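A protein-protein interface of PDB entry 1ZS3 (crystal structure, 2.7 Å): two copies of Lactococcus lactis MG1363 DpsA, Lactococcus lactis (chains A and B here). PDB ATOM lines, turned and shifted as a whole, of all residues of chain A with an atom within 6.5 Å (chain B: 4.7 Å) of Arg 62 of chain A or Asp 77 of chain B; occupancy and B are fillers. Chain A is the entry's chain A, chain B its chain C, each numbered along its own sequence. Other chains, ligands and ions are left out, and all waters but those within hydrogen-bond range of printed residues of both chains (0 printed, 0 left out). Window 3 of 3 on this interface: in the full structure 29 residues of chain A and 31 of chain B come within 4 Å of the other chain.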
ATOM      1  N   LEU A  45     -34.694   2.138 -20.691  1.00  0.00           N
ATOM      2  CA  LEU A  45     -34.285   3.511 -20.418  1.00  0.00           C
ATOM      3  C   LEU A  45     -32.811   3.575 -20.486  1.00  0.00           C
ATOM      4  O   LEU A  45     -32.279   4.592 -20.878  1.00  0.00           O
ATOM      5  CB  LEU A  45     -34.735   3.964 -19.020  1.00  0.00           C
ATOM      6  CG  LEU A  45     -36.242   4.256 -18.908  1.00  0.00           C
ATOM      7  CD1 LEU A  45     -36.723   4.206 -17.497  1.00  0.00           C
ATOM      8  CD2 LEU A  45     -36.595   5.615 -19.554  1.00  0.00           C
ATOM      9  N   THR A  46     -32.115   2.506 -20.080  1.00  0.00           N
ATOM     10  CA  THR A  46     -30.710   2.352 -20.372  1.00  0.00           C
ATOM     11  C   THR A  46     -30.417   2.368 -21.873  1.00  0.00           C
ATOM     12  O   THR A  46     -29.457   3.015 -22.319  1.00  0.00           O
ATOM     13  CB  THR A  46     -30.202   1.054 -19.799  1.00  0.00           C
ATOM     14  OG1 THR A  46     -30.278   1.092 -18.367  1.00  0.00           O
ATOM     15  CG2 THR A  46     -28.730   0.877 -20.076  1.00  0.00           C
ATOM     16  N   ALA A  48     -32.366   3.739 -24.315  1.00  0.00           N
ATOM     17  CA  ALA A  48     -32.694   5.093 -24.791  1.00  0.00           C
ATOM     18  C   ALA A  48     -31.684   6.161 -24.292  1.00  0.00           C
ATOM     19  O   ALA A  48     -31.392   7.136 -24.975  1.00  0.00           O
ATOM     20  CB  ALA A  48     -34.150   5.452 -24.394  1.00  0.00           C
ATOM     21  N   GLY A  49     -31.122   5.905 -23.110  1.00  0.00           N
ATOM     22  CA  GLY A  49     -30.204   6.814 -22.449  1.00  0.00           C
ATOM     23  C   GLY A  49     -28.902   6.794 -23.189  1.00  0.00           C
ATOM     24  O   GLY A  49     -28.055   7.634 -22.946  1.00  0.00           O
ATOM     25  N   ILE A  50     -28.742   5.784 -24.050  1.00  0.00           N
ATOM     26  CA  ILE A  50     -27.550   5.578 -24.851  1.00  0.00           C
ATOM     27  C   ILE A  50     -27.662   6.018 -26.317  1.00  0.00           C
ATOM     28  O   ILE A  50     -26.702   6.532 -26.859  1.00  0.00           O
ATOM     29  CB  ILE A  50     -27.093   4.107 -24.758  1.00  0.00           C
ATOM     30  CG1 ILE A  50     -26.426   3.857 -23.423  1.00  0.00           C
ATOM     31  CG2 ILE A  50     -26.116   3.742 -25.869  1.00  0.00           C
ATOM     32  CD1 ILE A  50     -26.012   2.462 -23.207  1.00  0.00           C
ATOM     33  N   TYR A  51     -28.825   5.850 -26.915  1.00  0.00           N
ATOM     34  CA  TYR A  51     -28.957   6.046 -28.391  1.00  0.00           C
ATOM     35  C   TYR A  51     -29.747   7.281 -28.765  1.00  0.00           C
ATOM     36  O   TYR A  51     -29.816   7.620 -29.931  1.00  0.00           O
ATOM     37  CB  TYR A  51     -29.617   4.811 -29.073  1.00  0.00           C
ATOM     38  CG  TYR A  51     -28.673   3.617 -29.229  1.00  0.00           C
ATOM     39  CD1 TYR A  51     -27.657   3.657 -30.152  1.00  0.00           C
ATOM     40  CD2 TYR A  51     -28.782   2.481 -28.416  1.00  0.00           C
ATOM     41  CE1 TYR A  51     -26.785   2.603 -30.308  1.00  0.00           C
ATOM     42  CE2 TYR A  51     -27.911   1.418 -28.553  1.00  0.00           C
ATOM     43  CZ  TYR A  51     -26.908   1.489 -29.508  1.00  0.00           C
ATOM     44  OH  TYR A  51     -26.023   0.453 -29.673  1.00  0.00           O
ATOM     45  N   LYS A  57     -31.803  15.003 -23.228  1.00  0.00           N
ATOM     46  CA  LYS A  57     -32.717  13.860 -23.039  1.00  0.00           C
ATOM     47  C   LYS A  57     -31.968  12.594 -22.589  1.00  0.00           C
ATOM     48  O   LYS A  57     -32.488  11.814 -21.823  1.00  0.00           O
ATOM     49  CB  LYS A  57     -33.551  13.634 -24.297  1.00  0.00           C
ATOM     50  CG  LYS A  57     -34.179  14.916 -24.823  1.00  0.00           C
ATOM     51  CD  LYS A  57     -35.231  14.636 -25.857  1.00  0.00           C
ATOM     52  CE  LYS A  57     -36.137  15.873 -26.075  1.00  0.00           C
ATOM     53  NZ  LYS A  57     -35.869  16.572 -27.380  1.00  0.00           N
ATOM     54  N   CYS A  58     -30.717  12.435 -23.000  1.00  0.00           N
ATOM     55  CA  CYS A  58     -29.917  11.316 -22.522  1.00  0.00           C
ATOM     56  C   CYS A  58     -29.602  11.347 -21.037  1.00  0.00           C
ATOM     57  O   CYS A  58     -29.599  10.276 -20.424  1.00  0.00           O
ATOM     58  CB  CYS A  58     -28.605  11.180 -23.307  1.00  0.00           C
ATOM     59  SG  CYS A  58     -28.832  10.619 -25.005  1.00  0.00           S
ATOM     60  N   GLU A  59     -29.278  12.522 -20.485  1.00  0.00           N
ATOM     61  CA  GLU A  59     -28.928  12.668 -19.072  1.00  0.00           C
ATOM     62  C   GLU A  59     -30.171  12.419 -18.234  1.00  0.00           C
ATOM     63  O   GLU A  59     -30.109  11.746 -17.202  1.00  0.00           O
ATOM     64  CB  GLU A  59     -28.382  14.065 -18.810  1.00  0.00           C
ATOM     65  CG  GLU A  59     -27.467  14.210 -17.565  1.00  0.00           C
ATOM     66  CD  GLU A  59     -27.398  15.656 -16.999  1.00  0.00           C
ATOM     67  OE1 GLU A  59     -28.398  16.170 -16.402  1.00  0.00           O
ATOM     68  OE2 GLU A  59     -26.294  16.268 -17.143  1.00  0.00           O
ATOM     69  N   TYR A  60     -31.308  12.897 -18.748  1.00  0.00           N
ATOM     70  CA  TYR A  60     -32.604  12.795 -18.100  1.00  0.00           C
ATOM     71  C   TYR A  60     -33.095  11.365 -18.068  1.00  0.00           C
ATOM     72  O   TYR A  60     -33.596  10.881 -17.053  1.00  0.00           O
ATOM     73  CB  TYR A  60     -33.646  13.663 -18.844  1.00  0.00           C
ATOM     74  CG  TYR A  60     -34.963  13.704 -18.151  1.00  0.00           C
ATOM     75  CD1 TYR A  60     -35.037  13.794 -16.740  1.00  0.00           C
ATOM     76  CD2 TYR A  60     -36.144  13.572 -18.863  1.00  0.00           C
ATOM     77  CE1 TYR A  60     -36.271  13.790 -16.054  1.00  0.00           C
ATOM     78  CE2 TYR A  60     -37.423  13.585 -18.184  1.00  0.00           C
ATOM     79  CZ  TYR A  60     -37.465  13.691 -16.767  1.00  0.00           C
ATOM     80  OH  TYR A  60     -38.662  13.703 -16.054  1.00  0.00           O
ATOM     81  N   LEU A  61     -32.975  10.640 -19.187  1.00  0.00           N
ATOM     82  CA  LEU A  61     -33.445   9.263 -19.284  1.00  0.00           C
ATOM     83  C   LEU A  61     -32.612   8.344 -18.424  1.00  0.00           C
ATOM     84  O   LEU A  61     -33.161   7.452 -17.830  1.00  0.00           O
ATOM     85  CB  LEU A  61     -33.472   8.770 -20.736  1.00  0.00           C
ATOM     86  CG  LEU A  61     -34.441   9.503 -21.690  1.00  0.00           C
ATOM     87  CD1 LEU A  61     -34.036   9.179 -23.136  1.00  0.00           C
ATOM     88  CD2 LEU A  61     -35.898   9.150 -21.494  1.00  0.00           C
ATOM     89  N   ARG A  62     -31.297   8.591 -18.350  1.00  0.00           N
ATOM     90  CA  ARG A  62     -30.375   7.832 -17.481  1.00  0.00           C
ATOM     91  C   ARG A  62     -30.690   8.046 -16.012  1.00  0.00           C
ATOM     92  O   ARG A  62     -30.363   7.214 -15.175  1.00  0.00           O
ATOM     93  CB  ARG A  62     -28.928   8.278 -17.685  1.00  0.00           C
ATOM     94  CG  ARG A  62     -28.290   7.770 -18.948  1.00  0.00           C
ATOM     95  CD  ARG A  62     -26.792   7.936 -19.064  1.00  0.00           C
ATOM     96  NE  ARG A  62     -26.403   7.954 -20.461  1.00  0.00           N
ATOM     97  CZ  ARG A  62     -25.187   7.799 -20.908  1.00  0.00           C
ATOM     98  NH1 ARG A  62     -24.159   7.627 -20.069  1.00  0.00           N
ATOM     99  NH2 ARG A  62     -24.940   7.820 -22.203  1.00  0.00           N
ATOM    100  N   GLU A  63     -31.271   9.195 -15.713  1.00  0.00           N
ATOM    101  CA  GLU A  63     -31.722   9.529 -14.352  1.00  0.00           C
ATOM    102  C   GLU A  63     -32.925   8.678 -13.996  1.00  0.00           C
ATOM    103  O   GLU A  63     -32.979   8.087 -12.925  1.00  0.00           O
ATOM    104  CB  GLU A  63     -32.020  11.023 -14.188  1.00  0.00           C
ATOM    105  CG  GLU A  63     -31.078  11.733 -13.214  1.00  0.00           C
ATOM    106  CD  GLU A  63     -31.863  12.762 -12.377  1.00  0.00           C
ATOM    107  OE1 GLU A  63     -32.294  12.382 -11.234  1.00  0.00           O
ATOM    108  OE2 GLU A  63     -32.058  13.949 -12.853  1.00  0.00           O
ATOM    109  N   ILE A  64     -33.873   8.584 -14.923  1.00  0.00           N
ATOM    110  CA  ILE A  64     -35.048   7.754 -14.739  1.00  0.00           C
ATOM    111  C   ILE A  64     -34.667   6.261 -14.597  1.00  0.00           C
ATOM    112  O   ILE A  64     -35.305   5.570 -13.846  1.00  0.00           O
ATOM    113  CB  ILE A  64     -36.080   7.979 -15.853  1.00  0.00           C
ATOM    114  CG1 ILE A  64     -36.550   9.443 -15.848  1.00  0.00           C
ATOM    115  CG2 ILE A  64     -37.298   7.053 -15.689  1.00  0.00           C
ATOM    116  CD1 ILE A  64     -37.167   9.886 -17.099  1.00  0.00           C
ATOM    117  N   ALA A  65     -33.649   5.780 -15.322  1.00  0.00           N
ATOM    118  CA  ALA A  65     -33.106   4.449 -15.137  1.00  0.00           C
ATOM    119  C   ALA A  65     -32.638   4.256 -13.676  1.00  0.00           C
ATOM    120  O   ALA A  65     -33.041   3.286 -13.053  1.00  0.00           O
ATOM    121  CB  ALA A  65     -32.016   4.178 -16.109  1.00  0.00           C
ATOM    122  N   GLN A  66     -31.806   5.159 -13.159  1.00  0.00           N
ATOM    123  CA  GLN A  66     -31.268   5.018 -11.807  1.00  0.00           C
ATOM    124  C   GLN A  66     -32.345   5.043 -10.733  1.00  0.00           C
ATOM    125  O   GLN A  66     -32.194   4.404  -9.683  1.00  0.00           O
ATOM    126  CB  GLN A  66     -30.189   6.100 -11.528  1.00  0.00           C
ATOM    127  CG  GLN A  66     -29.009   5.486 -10.752  1.00  0.00           C
ATOM    128  CD  GLN A  66     -28.611   6.264  -9.451  1.00  0.00           C
ATOM    129  OE1 GLN A  66     -28.355   5.633  -8.397  1.00  0.00           O
ATOM    130  NE2 GLN A  66     -28.549   7.614  -9.567  1.00  0.00           N
ATOM    131  N   ARG A  67     -33.441   5.751 -11.010  1.00  0.00           N
ATOM    132  CA  ARG A  67     -34.517   5.833 -10.064  1.00  0.00           C
ATOM    133  C   ARG A  67     -35.317   4.536 -10.050  1.00  0.00           C
ATOM    134  O   ARG A  67     -35.862   4.152  -9.005  1.00  0.00           O
ATOM    135  CB  ARG A  67     -35.455   7.013 -10.376  1.00  0.00           C
ATOM    136  CG  ARG A  67     -34.813   8.409 -10.376  1.00  0.00           C
ATOM    137  CD  ARG A  67     -34.399   8.971  -9.015  1.00  0.00           C
ATOM    138  NE  ARG A  67     -35.539   9.683  -8.448  1.00  0.00           N
ATOM    139  CZ  ARG A  67     -36.263   9.282  -7.394  1.00  0.00           C
ATOM    140  NH1 ARG A  67     -37.307  10.023  -6.999  1.00  0.00           N
ATOM    141  NH2 ARG A  67     -35.947   8.176  -6.721  1.00  0.00           N
ATOM    142  N   PHE B  73     -22.056   1.973 -18.759  1.00  0.00           N
ATOM    143  CA  PHE B  73     -22.379   3.266 -19.358  1.00  0.00           C
ATOM    144  C   PHE B  73     -21.139   3.938 -19.885  1.00  0.00           C
ATOM    145  O   PHE B  73     -21.151   4.473 -20.993  1.00  0.00           O
ATOM    146  CB  PHE B  73     -23.107   4.147 -18.348  1.00  0.00           C
ATOM    147  CG  PHE B  73     -24.613   4.022 -18.410  1.00  0.00           C
ATOM    148  CD1 PHE B  73     -25.328   3.667 -17.282  1.00  0.00           C
ATOM    149  CD2 PHE B  73     -25.306   4.300 -19.570  1.00  0.00           C
ATOM    150  CE1 PHE B  73     -26.676   3.567 -17.301  1.00  0.00           C
ATOM    151  CE2 PHE B  73     -26.666   4.182 -19.614  1.00  0.00           C
ATOM    152  CZ  PHE B  73     -27.362   3.820 -18.476  1.00  0.00           C
ATOM    153  N   LYS B  74     -20.059   3.854 -19.123  1.00  0.00           N
ATOM    154  CA  LYS B  74     -18.832   4.506 -19.501  1.00  0.00           C
ATOM    155  C   LYS B  74     -18.298   3.941 -20.796  1.00  0.00           C
ATOM    156  O   LYS B  74     -17.912   4.705 -21.674  1.00  0.00           O
ATOM    157  CB  LYS B  74     -17.815   4.381 -18.375  1.00  0.00           C
ATOM    158  CG  LYS B  74     -16.396   4.867 -18.741  1.00  0.00           C
ATOM    159  CD  LYS B  74     -15.352   4.440 -17.650  1.00  0.00           C
ATOM    160  CE  LYS B  74     -14.511   5.596 -17.121  1.00  0.00           C
ATOM    161  NZ  LYS B  74     -13.207   5.053 -16.622  1.00  0.00           N
ATOM    162  N   ILE B  75     -18.298   2.610 -20.934  1.00  0.00           N
ATOM    163  CA  ILE B  75     -17.699   1.964 -22.079  1.00  0.00           C
ATOM    164  C   ILE B  75     -18.640   2.053 -23.230  1.00  0.00           C
ATOM    165  O   ILE B  75     -18.227   2.229 -24.348  1.00  0.00           O
ATOM    166  CB  ILE B  75     -17.297   0.527 -21.742  1.00  0.00           C
ATOM    167  CG1 ILE B  75     -16.094   0.542 -20.781  1.00  0.00           C
ATOM    168  CG2 ILE B  75     -16.932  -0.252 -22.986  1.00  0.00           C
ATOM    169  CD1 ILE B  75     -15.797  -0.812 -20.200  1.00  0.00           C
ATOM    170  N   SER B  76     -19.923   1.915 -22.971  1.00  0.00           N
ATOM    171  CA  SER B  76     -20.906   2.128 -24.020  1.00  0.00           C
ATOM    172  C   SER B  76     -20.735   3.494 -24.646  1.00  0.00           C
ATOM    173  O   SER B  76     -20.877   3.635 -25.855  1.00  0.00           O
ATOM    174  CB  SER B  76     -22.313   1.957 -23.490  1.00  0.00           C
ATOM    175  OG  SER B  76     -22.501   0.661 -22.965  1.00  0.00           O
ATOM    176  N   ASP B  77     -20.434   4.498 -23.811  1.00  0.00           N
ATOM    177  CA  ASP B  77     -20.193   5.884 -24.262  1.00  0.00           C
ATOM    178  C   ASP B  77     -18.939   5.960 -25.130  1.00  0.00           C
ATOM    179  O   ASP B  77     -18.970   6.593 -26.180  1.00  0.00           O
ATOM    180  CB  ASP B  77     -20.005   6.830 -23.077  1.00  0.00           C
ATOM    181  CG  ASP B  77     -21.296   7.392 -22.590  1.00  0.00           C
ATOM    182  OD1 ASP B  77     -21.312   7.840 -21.425  1.00  0.00           O
ATOM    183  OD2 ASP B  77     -22.368   7.391 -23.256  1.00  0.00           O
ATOM    184  N   LEU B  78     -17.814   5.434 -24.626  1.00  0.00           N
ATOM    185  CA  LEU B  78     -16.555   5.408 -25.352  1.00  0.00           C
ATOM    186  C   LEU B  78     -16.710   4.754 -26.748  1.00  0.00           C
ATOM    187  O   LEU B  78     -16.190   5.304 -27.734  1.00  0.00           O
ATOM    188  CB  LEU B  78     -15.510   4.667 -24.544  1.00  0.00           C
ATOM    189  CG  LEU B  78     -15.034   5.350 -23.264  1.00  0.00           C
ATOM    190  CD1 LEU B  78     -14.328   4.361 -22.333  1.00  0.00           C
ATOM    191  CD2 LEU B  78     -14.116   6.456 -23.598  1.00  0.00           C
ATOM    192  N   LEU B  79     -17.459   3.651 -26.825  1.00  0.00           N
ATOM    193  CA  LEU B  79     -17.764   2.979 -28.080  1.00  0.00           C
ATOM    194  C   LEU B  79     -18.570   3.833 -29.049  1.00  0.00           C
ATOM    195  O   LEU B  79     -18.123   3.981 -30.185  1.00  0.00           O
ATOM    196  CB  LEU B  79     -18.503   1.663 -27.840  1.00  0.00           C
ATOM    197  CG  LEU B  79     -17.591   0.506 -27.387  1.00  0.00           C
ATOM    198  CD1 LEU B  79     -18.401  -0.553 -26.631  1.00  0.00           C
ATOM    199  CD2 LEU B  79     -16.854  -0.116 -28.535  1.00  0.00           C
ATOM    200  N   LEU B  80     -19.734   4.335 -28.652  1.00  0.00           N
ATOM    201  CA  LEU B  80     -20.523   5.138 -29.563  1.00  0.00           C
ATOM    202  C   LEU B  80     -19.737   6.346 -30.002  1.00  0.00           C
ATOM    203  O   LEU B  80     -19.937   6.844 -31.118  1.00  0.00           O
ATOM    204  CB  LEU B  80     -21.837   5.590 -28.966  1.00  0.00           C
ATOM    205  CG  LEU B  80     -23.058   4.682 -29.115  1.00  0.00           C
ATOM    206  CD1 LEU B  80     -22.989   3.643 -28.045  1.00  0.00           C
ATOM    207  CD2 LEU B  80     -24.361   5.455 -28.995  1.00  0.00           C
ATOM    208  N   ASP B  81     -18.845   6.795 -29.128  1.00  0.00           N
ATOM    209  CA  ASP B  81     -17.932   7.913 -29.400  1.00  0.00           C
ATOM    210  C   ASP B  81     -17.103   7.612 -30.654  1.00  0.00           C
ATOM    211  O   ASP B  81     -16.909   8.484 -31.521  1.00  0.00           O
ATOM    212  CB  ASP B  81     -16.930   8.097 -28.247  1.00  0.00           C
ATOM    213  CG  ASP B  81     -17.381   9.097 -27.164  1.00  0.00           C
ATOM    214  OD1 ASP B  81     -18.528   9.629 -27.214  1.00  0.00           O
ATOM    215  OD2 ASP B  81     -16.557   9.426 -26.260  1.00  0.00           O
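Along chain A the printed residues that touch a printed residue of chain B span positions 46 to 62.
Along chain B the printed residues that touch a printed residue of chain A span positions 73 to 80.
Among the printed residues, 7 pairs touch across the chains.
Among the printed residues, Asp or Glu carboxylates within 4 Å of a Lys or Arg side-chain nitrogen of the other chain: Arg 62 of chain A with Asp 77 of chain B (2.8 Å).
Among the printed residues, merely in contact across the chains: Thr 46 of chain A with Phe 73 of chain B, Ile 50 of chain A with Phe 73 of chain B, Ile 50 of chain A with Ser 76 of chain B, Ile 50 of chain A with Leu 80 of chain B, Tyr 51 of chain A with Leu 80 of chain B and Arg 62 of chain A with Phe 73 of chain B.
Leu 45 of chain A touches none of the printed residues of chain B.
Of the printed residues of chain B, Thr 46 of chain A touches Phe 73 (3.6 Å).
Of the printed residues of chain B, Ile 50 of chain A touches Phe 73 (3.8 Å), Ser 76 (3.7 Å) and Leu 80 (3.3 Å).
Lys 57 of chain A touches none of the printed residues of chain B.
Of chain B, only Phe 73 (3.6 Å) and Asp 77 (2.8 Å) come within 4 Å of Arg 62 of chain A.
Printed residues of chain A within 4 Å of Phe 73 of chain B: Thr 46 (3.6 Å), Ile 50 (3.8 Å) and Arg 62 (3.6 Å).
Of the printed residues of chain A, Ser 76 of chain B touches Ile 50 (3.7 Å).
Asp 77 of chain B touches just one residue of chain A: Arg 62.
Printed residues of chain A within 4 Å of Leu 80 of chain B: Ile 50 (3.3 Å) and Tyr 51 (3.9 Å).
The nearest printed residue of chain B that does not touch Arg 62 of chain A is Lys 74 of chain B (5.7 Å).
The nearest printed residue of chain B that does not touch Thr 46 of chain A is Ser 76 of chain B (6.9 Å).
O of Gly 49 of chain A is in hydrogen-bond range of NE of Arg 62 of chain A (3.0 Å).
No position is printed for both chains.
Of the 7 pairs that touch across the chains among the printed residues, none has its exchanged pair printed and touching as well.
OD2 of Asp 77 of chain B lies within salt-bridge range of NH2 of Arg 62 of chain A (2.8 Å).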
